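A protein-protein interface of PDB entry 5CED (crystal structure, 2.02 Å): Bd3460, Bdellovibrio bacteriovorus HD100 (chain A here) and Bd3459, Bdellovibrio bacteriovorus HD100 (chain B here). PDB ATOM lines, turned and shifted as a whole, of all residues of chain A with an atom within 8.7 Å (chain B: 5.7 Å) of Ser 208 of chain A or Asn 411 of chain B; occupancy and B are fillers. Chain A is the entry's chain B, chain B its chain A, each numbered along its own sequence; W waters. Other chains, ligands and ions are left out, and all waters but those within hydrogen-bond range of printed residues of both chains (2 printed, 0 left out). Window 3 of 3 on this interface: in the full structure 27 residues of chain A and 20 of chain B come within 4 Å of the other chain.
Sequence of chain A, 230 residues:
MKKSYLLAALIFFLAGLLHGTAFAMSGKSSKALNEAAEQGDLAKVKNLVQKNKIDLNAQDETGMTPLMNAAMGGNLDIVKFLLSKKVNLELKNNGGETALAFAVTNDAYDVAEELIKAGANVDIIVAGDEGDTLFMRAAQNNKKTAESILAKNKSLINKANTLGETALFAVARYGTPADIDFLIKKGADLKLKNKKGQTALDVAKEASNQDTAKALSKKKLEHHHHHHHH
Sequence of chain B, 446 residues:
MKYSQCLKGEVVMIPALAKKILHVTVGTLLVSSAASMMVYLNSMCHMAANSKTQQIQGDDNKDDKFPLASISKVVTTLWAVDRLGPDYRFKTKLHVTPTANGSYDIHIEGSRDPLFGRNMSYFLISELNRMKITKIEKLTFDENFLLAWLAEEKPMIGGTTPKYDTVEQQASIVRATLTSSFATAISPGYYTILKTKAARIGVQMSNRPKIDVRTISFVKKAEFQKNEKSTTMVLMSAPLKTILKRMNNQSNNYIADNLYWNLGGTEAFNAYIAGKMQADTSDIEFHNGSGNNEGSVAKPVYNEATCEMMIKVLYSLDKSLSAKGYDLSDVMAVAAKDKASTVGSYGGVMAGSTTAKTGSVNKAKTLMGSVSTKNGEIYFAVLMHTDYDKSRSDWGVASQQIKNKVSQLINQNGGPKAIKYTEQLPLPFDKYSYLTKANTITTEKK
Of the printed residues of chain B, Gly 175 of chain A touches Val 349 (3.3 Å). Of the printed residues of chain B, Ala 207 of chain A touches Gln 408 (3.2 Å) and Asn 411 (3.1 Å). Of the printed residues of chain B, Asn 209 of chain A touches Asn 411 (3.6 Å). Of the printed residues of chain A, Ser 407 of chain B touches Tyr 174. Of the printed residues of chain A, Gln 408 of chain B touches Tyr 174 and Ala 207. Printed residues of chain A within 4 Å of Asn 411 of chain B: Arg 173 (3.0 Å), Ala 207 (3.1 Å), Ser 208 (3.4 Å) and Asn 209 (3.6 Å). Gly 414 of chain B touches none of the printed residues of chain A. Gly 415 of chain B touches none of the printed residues of chain A. The nearest printed residue of chain B that does not touch Tyr 174 of chain A is Asn 411 of chain B (4.01 Å).
Water W2 lies within hydrogen-bond range of OE1 of Gln 408 of chain B (2.4 Å) and OH of Tyr 174 of chain A (2.7 Å). Water W1 lies within hydrogen-bond range of O of Asn 411 of chain B (3.2 Å), O of Ser 208 of chain A (3.2 Å) and N of Gln 210 of chain A (3.2 Å).
The backbone carbonyl oxygen of Arg 173 of chain A sits at hydrogen-bond distance from the side-chain amide nitrogen of Asn 411 of chain B (3.0 Å). The backbone carbonyl oxygen of Ser 208 of chain A sits close to the backbone carbonyl oxygen of Asn 411 of chain B (3.4 Å). ND2 of Asn 411 of chain B is in hydrogen-bond range of O of Ala 207 of chain A, 3.1 Å away. The backbone carbonyl oxygen (O) of Ala 207 of chain A is in hydrogen-bond range of the side-chain amide nitrogen (NE2) of Gln 408 of chain B. The backbone NH (N) of Val 349 of chain B sits at hydrogen-bond distance from the backbone carbonyl oxygen (O) of Tyr 174 of chain A (3.2 Å).
Tyr 174 of chain A touches Ser 407 of chain B. Tyr 174 of chain A touches Gln 408 of chain B (CE1 to OE1, 3.8 Å). O of Gly 175 of chain A touches CG1 of Val 349 of chain B, at 3.3 Å. Asn 411 of chain B touches Asn 209 of chain A.
Of the 20 printed residues of chain A, 6 touch a printed residue of chain B. Printed residues of chain B that touch a printed residue of chain A: Val 349, Ser 407, Gln 408 and Asn 411. Hydrophobic or aromatic side chains of chain B that line the printed part of chain A: Val 349. Among the printed residues, no Asp or Glu carboxylate lies within 4 Å of a Lys or Arg side-chain nitrogen of the other chain.
The side-chain amide nitrogen (ND2) of Asn 209 of chain A is in hydrogen-bond range of the backbone carbonyl oxygen (O) of Gly 175 of chain A. The side-chain amide nitrogen (NE2) of Gln 408 of chain B lies close to the side-chain amide nitrogen (NE2) of Gln 412 of chain B, at 3.0 Å. N of Thr 212 of chain A is in hydrogen-bond range of OD1 of Asn 209 of chain A (3.2 Å). The side-chain amide oxygen (OD1) of Asn 209 of chain A sits close to the backbone NH (N) of Asp 211 of chain A. O of Ala 172 of chain A sits at hydrogen-bond distance from ND2 of Asn 209 of chain A, at 3.3 Å. O of Arg 173 of chain A lies within hydrogen-bond range of ND2 of Asn 209 of chain A, 3.0 Å away.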
ATOM      1  N   ALA A 170      -1.175  22.983   9.020  1.00  0.00           N
ATOM      2  CA  ALA A 170      -2.585  23.222   8.845  1.00  0.00           C
ATOM      3  C   ALA A 170      -2.792  24.314   7.771  1.00  0.00           C
ATOM      4  O   ALA A 170      -3.685  24.250   6.930  1.00  0.00           O
ATOM      5  CB  ALA A 170      -3.218  23.657  10.166  1.00  0.00           C
ATOM      6  N   VAL A 171      -1.992  25.354   7.864  1.00  0.00           N
ATOM      7  CA  VAL A 171      -2.059  26.470   6.957  1.00  0.00           C
ATOM      8  C   VAL A 171      -1.522  26.080   5.583  1.00  0.00           C
ATOM      9  O   VAL A 171      -2.059  26.548   4.559  1.00  0.00           O
ATOM     10  CB  VAL A 171      -1.288  27.638   7.573  1.00  0.00           C
ATOM     11  CG1 VAL A 171      -0.923  28.654   6.545  1.00  0.00           C
ATOM     12  CG2 VAL A 171      -2.154  28.259   8.693  1.00  0.00           C
ATOM     13  N   ALA A 172      -0.522  25.201   5.542  1.00  0.00           N
ATOM     14  CA  ALA A 172      -0.049  24.662   4.262  1.00  0.00           C
ATOM     15  C   ALA A 172      -1.219  23.986   3.542  1.00  0.00           C
ATOM     16  O   ALA A 172      -1.412  24.155   2.335  1.00  0.00           O
ATOM     17  CB  ALA A 172       1.118  23.700   4.438  1.00  0.00           C
ATOM     18  N   ARG A 173      -2.028  23.244   4.282  1.00  0.00           N
ATOM     19  CA  ARG A 173      -3.163  22.605   3.636  1.00  0.00           C
ATOM     20  C   ARG A 173      -4.240  23.581   3.216  1.00  0.00           C
ATOM     21  O   ARG A 173      -4.694  23.515   2.085  1.00  0.00           O
ATOM     22  CB  ARG A 173      -3.817  21.564   4.529  1.00  0.00           C
ATOM     23  CG  ARG A 173      -3.004  20.323   4.713  1.00  0.00           C
ATOM     24  CD  ARG A 173      -3.820  19.170   5.248  1.00  0.00           C
ATOM     25  NE  ARG A 173      -3.019  17.986   5.502  1.00  0.00           N
ATOM     26  CZ  ARG A 173      -2.333  17.749   6.638  1.00  0.00           C
ATOM     27  NH1 ARG A 173      -2.320  18.623   7.632  1.00  0.00           N
ATOM     28  NH2 ARG A 173      -1.646  16.627   6.772  1.00  0.00           N
ATOM     29  N   TYR A 174      -4.702  24.414   4.169  1.00  0.00           N
ATOM     30  CA  TYR A 174      -5.981  25.120   4.056  1.00  0.00           C
ATOM     31  C   TYR A 174      -5.899  26.629   4.132  1.00  0.00           C
ATOM     32  O   TYR A 174      -6.937  27.322   4.132  1.00  0.00           O
ATOM     33  CB  TYR A 174      -6.984  24.559   5.097  1.00  0.00           C
ATOM     34  CG  TYR A 174      -7.162  23.059   4.992  1.00  0.00           C
ATOM     35  CD1 TYR A 174      -7.525  22.468   3.794  1.00  0.00           C
ATOM     36  CD2 TYR A 174      -6.918  22.220   6.071  1.00  0.00           C
ATOM     37  CE1 TYR A 174      -7.713  21.096   3.677  1.00  0.00           C
ATOM     38  CE2 TYR A 174      -7.047  20.841   5.952  1.00  0.00           C
ATOM     39  CZ  TYR A 174      -7.465  20.289   4.776  1.00  0.00           C
ATOM     40  OH  TYR A 174      -7.587  18.939   4.681  1.00  0.00           O
ATOM     41  N   GLY A 175      -4.678  27.154   4.180  1.00  0.00           N
ATOM     42  CA  GLY A 175      -4.460  28.576   4.288  1.00  0.00           C
ATOM     43  C   GLY A 175      -3.864  29.227   3.065  1.00  0.00           C
ATOM     44  O   GLY A 175      -3.911  28.670   1.960  1.00  0.00           O
ATOM     45  N   THR A 176      -3.333  30.436   3.279  1.00  0.00           N
ATOM     46  CA  THR A 176      -2.831  31.316   2.256  1.00  0.00           C
ATOM     47  C   THR A 176      -1.333  31.592   2.451  1.00  0.00           C
ATOM     48  O   THR A 176      -0.797  31.378   3.559  1.00  0.00           O
ATOM     49  CB  THR A 176      -3.498  32.696   2.380  1.00  0.00           C
ATOM     50  OG1 THR A 176      -3.203  33.226   3.696  1.00  0.00           O
ATOM     51  CG2 THR A 176      -5.030  32.621   2.178  1.00  0.00           C
ATOM     52  N   LEU A 201       5.469  21.451   3.114  1.00  0.00           N
ATOM     53  CA  LEU A 201       5.389  21.502   1.638  1.00  0.00           C
ATOM     54  C   LEU A 201       4.707  20.226   1.101  1.00  0.00           C
ATOM     55  O   LEU A 201       3.842  20.289   0.207  1.00  0.00           O
ATOM     56  CB  LEU A 201       6.801  21.627   1.023  1.00  0.00           C
ATOM     57  CG  LEU A 201       6.933  21.608  -0.508  1.00  0.00           C
ATOM     58  CD1 LEU A 201       6.013  22.674  -1.137  1.00  0.00           C
ATOM     59  CD2 LEU A 201       8.391  21.827  -0.921  1.00  0.00           C
ATOM     60  N   ASP A 202       5.116  19.073   1.619  1.00  0.00           N
ATOM     61  CA  ASP A 202       4.492  17.815   1.200  1.00  0.00           C
ATOM     62  C   ASP A 202       2.978  17.828   1.399  1.00  0.00           C
ATOM     63  O   ASP A 202       2.200  17.384   0.528  1.00  0.00           O
ATOM     64  CB  ASP A 202       5.042  16.674   1.997  1.00  0.00           C
ATOM     65  CG  ASP A 202       6.422  16.283   1.580  1.00  0.00           C
ATOM     66  OD1 ASP A 202       6.810  16.494   0.401  1.00  0.00           O
ATOM     67  OD2 ASP A 202       7.123  15.787   2.471  1.00  0.00           O
ATOM     68  N   VAL A 203       2.529  18.304   2.541  1.00  0.00           N
ATOM     69  CA  VAL A 203       1.074  18.275   2.778  1.00  0.00           C
ATOM     70  C   VAL A 203       0.324  19.322   1.957  1.00  0.00           C
ATOM     71  O   VAL A 203      -0.840  19.142   1.635  1.00  0.00           O
ATOM     72  CB  VAL A 203       0.702  18.348   4.275  1.00  0.00           C
ATOM     73  CG1 VAL A 203       1.443  17.245   5.069  1.00  0.00           C
ATOM     74  CG2 VAL A 203       0.910  19.741   4.878  1.00  0.00           C
ATOM     75  N   ALA A 204       0.978  20.427   1.650  1.00  0.00           N
ATOM     76  CA  ALA A 204       0.397  21.444   0.757  1.00  0.00           C
ATOM     77  C   ALA A 204       0.127  20.809  -0.591  1.00  0.00           C
ATOM     78  O   ALA A 204      -0.976  20.959  -1.129  1.00  0.00           O
ATOM     79  CB  ALA A 204       1.289  22.676   0.631  1.00  0.00           C
ATOM     80  N   LYS A 205       1.083  20.034  -1.112  1.00  0.00           N
ATOM     81  CA  LYS A 205       0.873  19.454  -2.418  1.00  0.00           C
ATOM     82  C   LYS A 205      -0.247  18.389  -2.388  1.00  0.00           C
ATOM     83  O   LYS A 205      -1.130  18.351  -3.258  1.00  0.00           O
ATOM     84  CB  LYS A 205       2.163  18.841  -2.933  1.00  0.00           C
ATOM     85  CG  LYS A 205       3.318  19.824  -3.098  1.00  0.00           C
ATOM     86  CD  LYS A 205       4.444  19.052  -3.760  1.00  0.00           C
ATOM     87  CE  LYS A 205       5.774  19.293  -3.191  1.00  0.00           C
ATOM     88  NZ  LYS A 205       6.778  18.451  -3.889  1.00  0.00           N
ATOM     89  N   GLU A 206      -0.228  17.554  -1.352  1.00  0.00           N
ATOM     90  CA  GLU A 206      -1.216  16.505  -1.192  1.00  0.00           C
ATOM     91  C   GLU A 206      -2.619  17.100  -1.111  1.00  0.00           C
ATOM     92  O   GLU A 206      -3.526  16.579  -1.679  1.00  0.00           O
ATOM     93  CB  GLU A 206      -0.869  15.673   0.045  1.00  0.00           C
ATOM     94  CG  GLU A 206      -1.818  14.532   0.379  1.00  0.00           C
ATOM     95  CD  GLU A 206      -1.406  13.837   1.677  1.00  0.00           C
ATOM     96  OE1 GLU A 206      -1.087  14.521   2.691  1.00  0.00           O
ATOM     97  OE2 GLU A 206      -1.398  12.606   1.683  1.00  0.00           O
ATOM     98  N   ALA A 207      -2.763  18.270  -0.509  1.00  0.00           N
ATOM     99  CA  ALA A 207      -4.050  18.928  -0.409  1.00  0.00           C
ATOM    100  C   ALA A 207      -4.415  19.806  -1.606  1.00  0.00           C
ATOM    101  O   ALA A 207      -5.420  20.495  -1.548  1.00  0.00           O
ATOM    102  CB  ALA A 207      -4.079  19.763   0.868  1.00  0.00           C
ATOM    103  N   SER A 208      -3.610  19.786  -2.669  1.00  0.00           N
ATOM    104  CA  SER A 208      -3.810  20.596  -3.881  1.00  0.00           C
ATOM    105  C   SER A 208      -3.840  22.087  -3.622  1.00  0.00           C
ATOM    106  O   SER A 208      -4.552  22.791  -4.298  1.00  0.00           O
ATOM    107  CB  SER A 208      -5.092  20.205  -4.615  1.00  0.00           C
ATOM    108  OG  SER A 208      -5.080  18.839  -4.902  1.00  0.00           O
ATOM    109  N   ASN A 209      -3.109  22.549  -2.614  1.00  0.00           N
ATOM    110  CA  ASN A 209      -3.048  23.977  -2.338  1.00  0.00           C
ATOM    111  C   ASN A 209      -1.866  24.547  -3.083  1.00  0.00           C
ATOM    112  O   ASN A 209      -0.726  24.534  -2.588  1.00  0.00           O
ATOM    113  CB  ASN A 209      -2.913  24.267  -0.842  1.00  0.00           C
ATOM    114  CG  ASN A 209      -3.154  25.728  -0.519  1.00  0.00           C
ATOM    115  OD1 ASN A 209      -2.879  26.630  -1.343  1.00  0.00           O
ATOM    116  ND2 ASN A 209      -3.636  25.989   0.718  1.00  0.00           N
ATOM    117  N   GLN A 210      -2.150  25.007  -4.288  1.00  0.00           N
ATOM    118  CA  GLN A 210      -1.125  25.505  -5.212  1.00  0.00           C
ATOM    119  C   GLN A 210      -0.357  26.628  -4.640  1.00  0.00           C
ATOM    120  O   GLN A 210       0.865  26.621  -4.692  1.00  0.00           O
ATOM    121  CB  GLN A 210      -1.749  26.005  -6.507  1.00  0.00           C
ATOM    122  CG  GLN A 210      -1.990  24.892  -7.495  1.00  0.00           C
ATOM    123  CD  GLN A 210      -0.831  24.678  -8.461  1.00  0.00           C
ATOM    124  OE1 GLN A 210      -0.014  25.584  -8.735  1.00  0.00           O
ATOM    125  NE2 GLN A 210      -0.785  23.480  -9.029  1.00  0.00           N
ATOM    126  N   ASP A 211      -1.074  27.568  -4.068  1.00  0.00           N
ATOM    127  CA  ASP A 211      -0.487  28.812  -3.596  1.00  0.00           C
ATOM    128  C   ASP A 211       0.439  28.656  -2.400  1.00  0.00           C
ATOM    129  O   ASP A 211       1.493  29.263  -2.365  1.00  0.00           O
ATOM    130  CB  ASP A 211      -1.581  29.861  -3.280  1.00  0.00           C
ATOM    131  CG  ASP A 211      -2.308  30.331  -4.507  1.00  0.00           C
ATOM    132  OD1 ASP A 211      -1.645  30.627  -5.489  1.00  0.00           O
ATOM    133  OD2 ASP A 211      -3.544  30.446  -4.491  1.00  0.00           O
ATOM    134  N   THR A 212       0.059  27.859  -1.422  1.00  0.00           N
ATOM    135  CA  THR A 212       0.955  27.616  -0.303  1.00  0.00           C
ATOM    136  C   THR A 212       2.135  26.721  -0.718  1.00  0.00           C
ATOM    137  O   THR A 212       3.215  26.910  -0.207  1.00  0.00           O
ATOM    138  CB  THR A 212       0.228  26.984   0.934  1.00  0.00           C
ATOM    139  OG1 THR A 212      -0.397  25.750   0.537  1.00  0.00           O
ATOM    140  CG2 THR A 212      -0.816  27.946   1.496  1.00  0.00           C
ATOM    141  N   ALA A 213       1.923  25.704  -1.553  1.00  0.00           N
ATOM    142  CA  ALA A 213       3.053  24.869  -2.009  1.00  0.00           C
ATOM    143  C   ALA A 213       4.095  25.741  -2.695  1.00  0.00           C
ATOM    144  O   ALA A 213       5.281  25.652  -2.365  1.00  0.00           O
ATOM    145  CB  ALA A 213       2.620  23.714  -2.948  1.00  0.00           C
ATOM    146  N   VAL B 349      -8.203  30.139   3.123  1.00  0.00           N
ATOM    147  CA  VAL B 349      -8.638  30.417   1.750  1.00  0.00           C
ATOM    148  C   VAL B 349     -10.081  30.904   1.722  1.00  0.00           C
ATOM    149  O   VAL B 349     -10.481  31.586   0.797  1.00  0.00           O
ATOM    150  CB  VAL B 349      -8.433  29.186   0.820  1.00  0.00           C
ATOM    151  CG1 VAL B 349      -6.948  28.886   0.625  1.00  0.00           C
ATOM    152  CG2 VAL B 349      -9.154  27.958   1.310  1.00  0.00           C
ATOM    153  N   VAL B 406     -14.474  22.764   3.155  1.00  0.00           N
ATOM    154  CA  VAL B 406     -14.753  23.873   2.272  1.00  0.00           C
ATOM    155  C   VAL B 406     -13.433  24.400   1.691  1.00  0.00           C
ATOM    156  O   VAL B 406     -13.388  24.708   0.505  1.00  0.00           O
ATOM    157  CB  VAL B 406     -15.551  24.975   2.986  1.00  0.00           C
ATOM    158  CG1 VAL B 406     -15.735  26.207   2.095  1.00  0.00           C
ATOM    159  CG2 VAL B 406     -16.913  24.440   3.341  1.00  0.00           C
ATOM    160  N   SER B 407     -12.377  24.478   2.508  1.00  0.00           N
ATOM    161  CA  SER B 407     -11.057  24.921   2.028  1.00  0.00           C
ATOM    162  C   SER B 407     -10.537  23.982   0.943  1.00  0.00           C
ATOM    163  O   SER B 407      -9.924  24.423  -0.031  1.00  0.00           O
ATOM    164  CB  SER B 407     -10.059  25.009   3.185  1.00  0.00           C
ATOM    165  OG  SER B 407     -10.540  25.909   4.149  1.00  0.00           O
ATOM    166  N   GLN B 408     -10.797  22.693   1.106  1.00  0.00           N
ATOM    167  CA  GLN B 408     -10.380  21.702   0.106  1.00  0.00           C
ATOM    168  C   GLN B 408     -11.161  21.907  -1.205  1.00  0.00           C
ATOM    169  O   GLN B 408     -10.616  21.765  -2.286  1.00  0.00           O
ATOM    170  CB  GLN B 408     -10.568  20.254   0.651  1.00  0.00           C
ATOM    171  CG  GLN B 408     -10.108  19.142  -0.302  1.00  0.00           C
ATOM    172  CD  GLN B 408      -8.607  19.213  -0.581  1.00  0.00           C
ATOM    173  OE1 GLN B 408      -7.796  19.436   0.315  1.00  0.00           O
ATOM    174  NE2 GLN B 408      -8.237  19.067  -1.831  1.00  0.00           N
ATOM    175  N   LEU B 409     -12.449  22.222  -1.101  1.00  0.00           N
ATOM    176  CA  LEU B 409     -13.227  22.507  -2.304  1.00  0.00           C
ATOM    177  C   LEU B 409     -12.600  23.695  -3.079  1.00  0.00           C
ATOM    178  O   LEU B 409     -12.474  23.675  -4.327  1.00  0.00           O
ATOM    179  CB  LEU B 409     -14.688  22.747  -1.936  1.00  0.00           C
ATOM    180  CG  LEU B 409     -15.636  23.147  -3.075  1.00  0.00           C
ATOM    181  CD1 LEU B 409     -15.797  22.026  -4.120  1.00  0.00           C
ATOM    182  CD2 LEU B 409     -16.969  23.560  -2.490  1.00  0.00           C
ATOM    183  N   ILE B 410     -12.179  24.710  -2.356  1.00  0.00           N
ATOM    184  CA  ILE B 410     -11.557  25.884  -2.964  1.00  0.00           C
ATOM    185  C   ILE B 410     -10.216  25.493  -3.632  1.00  0.00           C
ATOM    186  O   ILE B 410     -10.008  25.783  -4.847  1.00  0.00           O
ATOM    187  CB  ILE B 410     -11.365  27.020  -1.934  1.00  0.00           C
ATOM    188  CG1 ILE B 410     -12.716  27.560  -1.505  1.00  0.00           C
ATOM    189  CG2 ILE B 410     -10.510  28.138  -2.511  1.00  0.00           C
ATOM    190  CD1 ILE B 410     -12.647  28.513  -0.348  1.00  0.00           C
ATOM    191  N   ASN B 411      -9.391  24.739  -2.891  1.00  0.00           N
ATOM    192  CA  ASN B 411      -8.090  24.242  -3.380  1.00  0.00           C
ATOM    193  C   ASN B 411      -8.269  23.515  -4.717  1.00  0.00           C
ATOM    194  O   ASN B 411      -7.508  23.729  -5.654  1.00  0.00           O
ATOM    195  CB  ASN B 411      -7.460  23.213  -2.393  1.00  0.00           C
ATOM    196  CG  ASN B 411      -6.905  23.833  -1.100  1.00  0.00           C
ATOM    197  OD1 ASN B 411      -6.692  25.042  -1.001  1.00  0.00           O
ATOM    198  ND2 ASN B 411      -6.647  22.956  -0.092  1.00  0.00           N
ATOM    199  N   GLN B 412      -9.268  22.642  -4.775  1.00  0.00           N
ATOM    200  CA  GLN B 412      -9.544  21.841  -5.969  1.00  0.00           C
ATOM    201  C   GLN B 412     -10.077  22.583  -7.194  1.00  0.00           C
ATOM    202  O   GLN B 412     -10.182  21.994  -8.264  1.00  0.00           O
ATOM    203  CB  GLN B 412     -10.482  20.691  -5.618  1.00  0.00           C
ATOM    204  CG  GLN B 412      -9.695  19.494  -5.108  1.00  0.00           C
ATOM    205  CD  GLN B 412     -10.542  18.543  -4.323  1.00  0.00           C
ATOM    206  OE1 GLN B 412     -11.736  18.731  -4.213  1.00  0.00           O
ATOM    207  NE2 GLN B 412      -9.925  17.519  -3.760  1.00  0.00           N
ATOM    208  N   ASN B 413     -10.409  23.851  -7.016  1.00  0.00           N
ATOM    209  CA  ASN B 413     -10.950  24.710  -8.043  1.00  0.00           C
ATOM    210  C   ASN B 413     -10.070  25.903  -8.283  1.00  0.00           C
ATOM    211  O   ASN B 413     -10.562  27.005  -8.610  1.00  0.00           O
ATOM    212  CB  ASN B 413     -12.312  25.165  -7.575  1.00  0.00           C
ATOM    213  CG  ASN B 413     -13.346  24.119  -7.805  1.00  0.00           C
ATOM    214  OD1 ASN B 413     -13.828  23.987  -8.922  1.00  0.00           O
ATOM    215  ND2 ASN B 413     -13.705  23.378  -6.770  1.00  0.00           N
ATOM    216  N   GLY B 414      -8.764  25.673  -8.114  1.00  0.00           N
ATOM    217  CA  GLY B 414      -7.722  26.632  -8.423  1.00  0.00           C
ATOM    218  C   GLY B 414      -7.497  27.691  -7.382  1.00  0.00           C
ATOM    219  O   GLY B 414      -6.845  28.691  -7.639  1.00  0.00           O
ATOM    220  N   GLY B 415      -8.052  27.500  -6.190  1.00  0.00           N
ATOM    221  CA  GLY B 415      -7.758  28.411  -5.120  1.00  0.00           C
ATOM    222  C   GLY B 415      -8.746  29.537  -5.103  1.00  0.00           C
ATOM    223  O   GLY B 415      -9.586  29.638  -5.992  1.00  0.00           O
HETATM  224  O   HOH W   1      -5.039  25.726  -5.582  1.00  0.00           O
HETATM  225  O   HOH W   2      -7.123  18.004   2.154  1.00  0.00           O
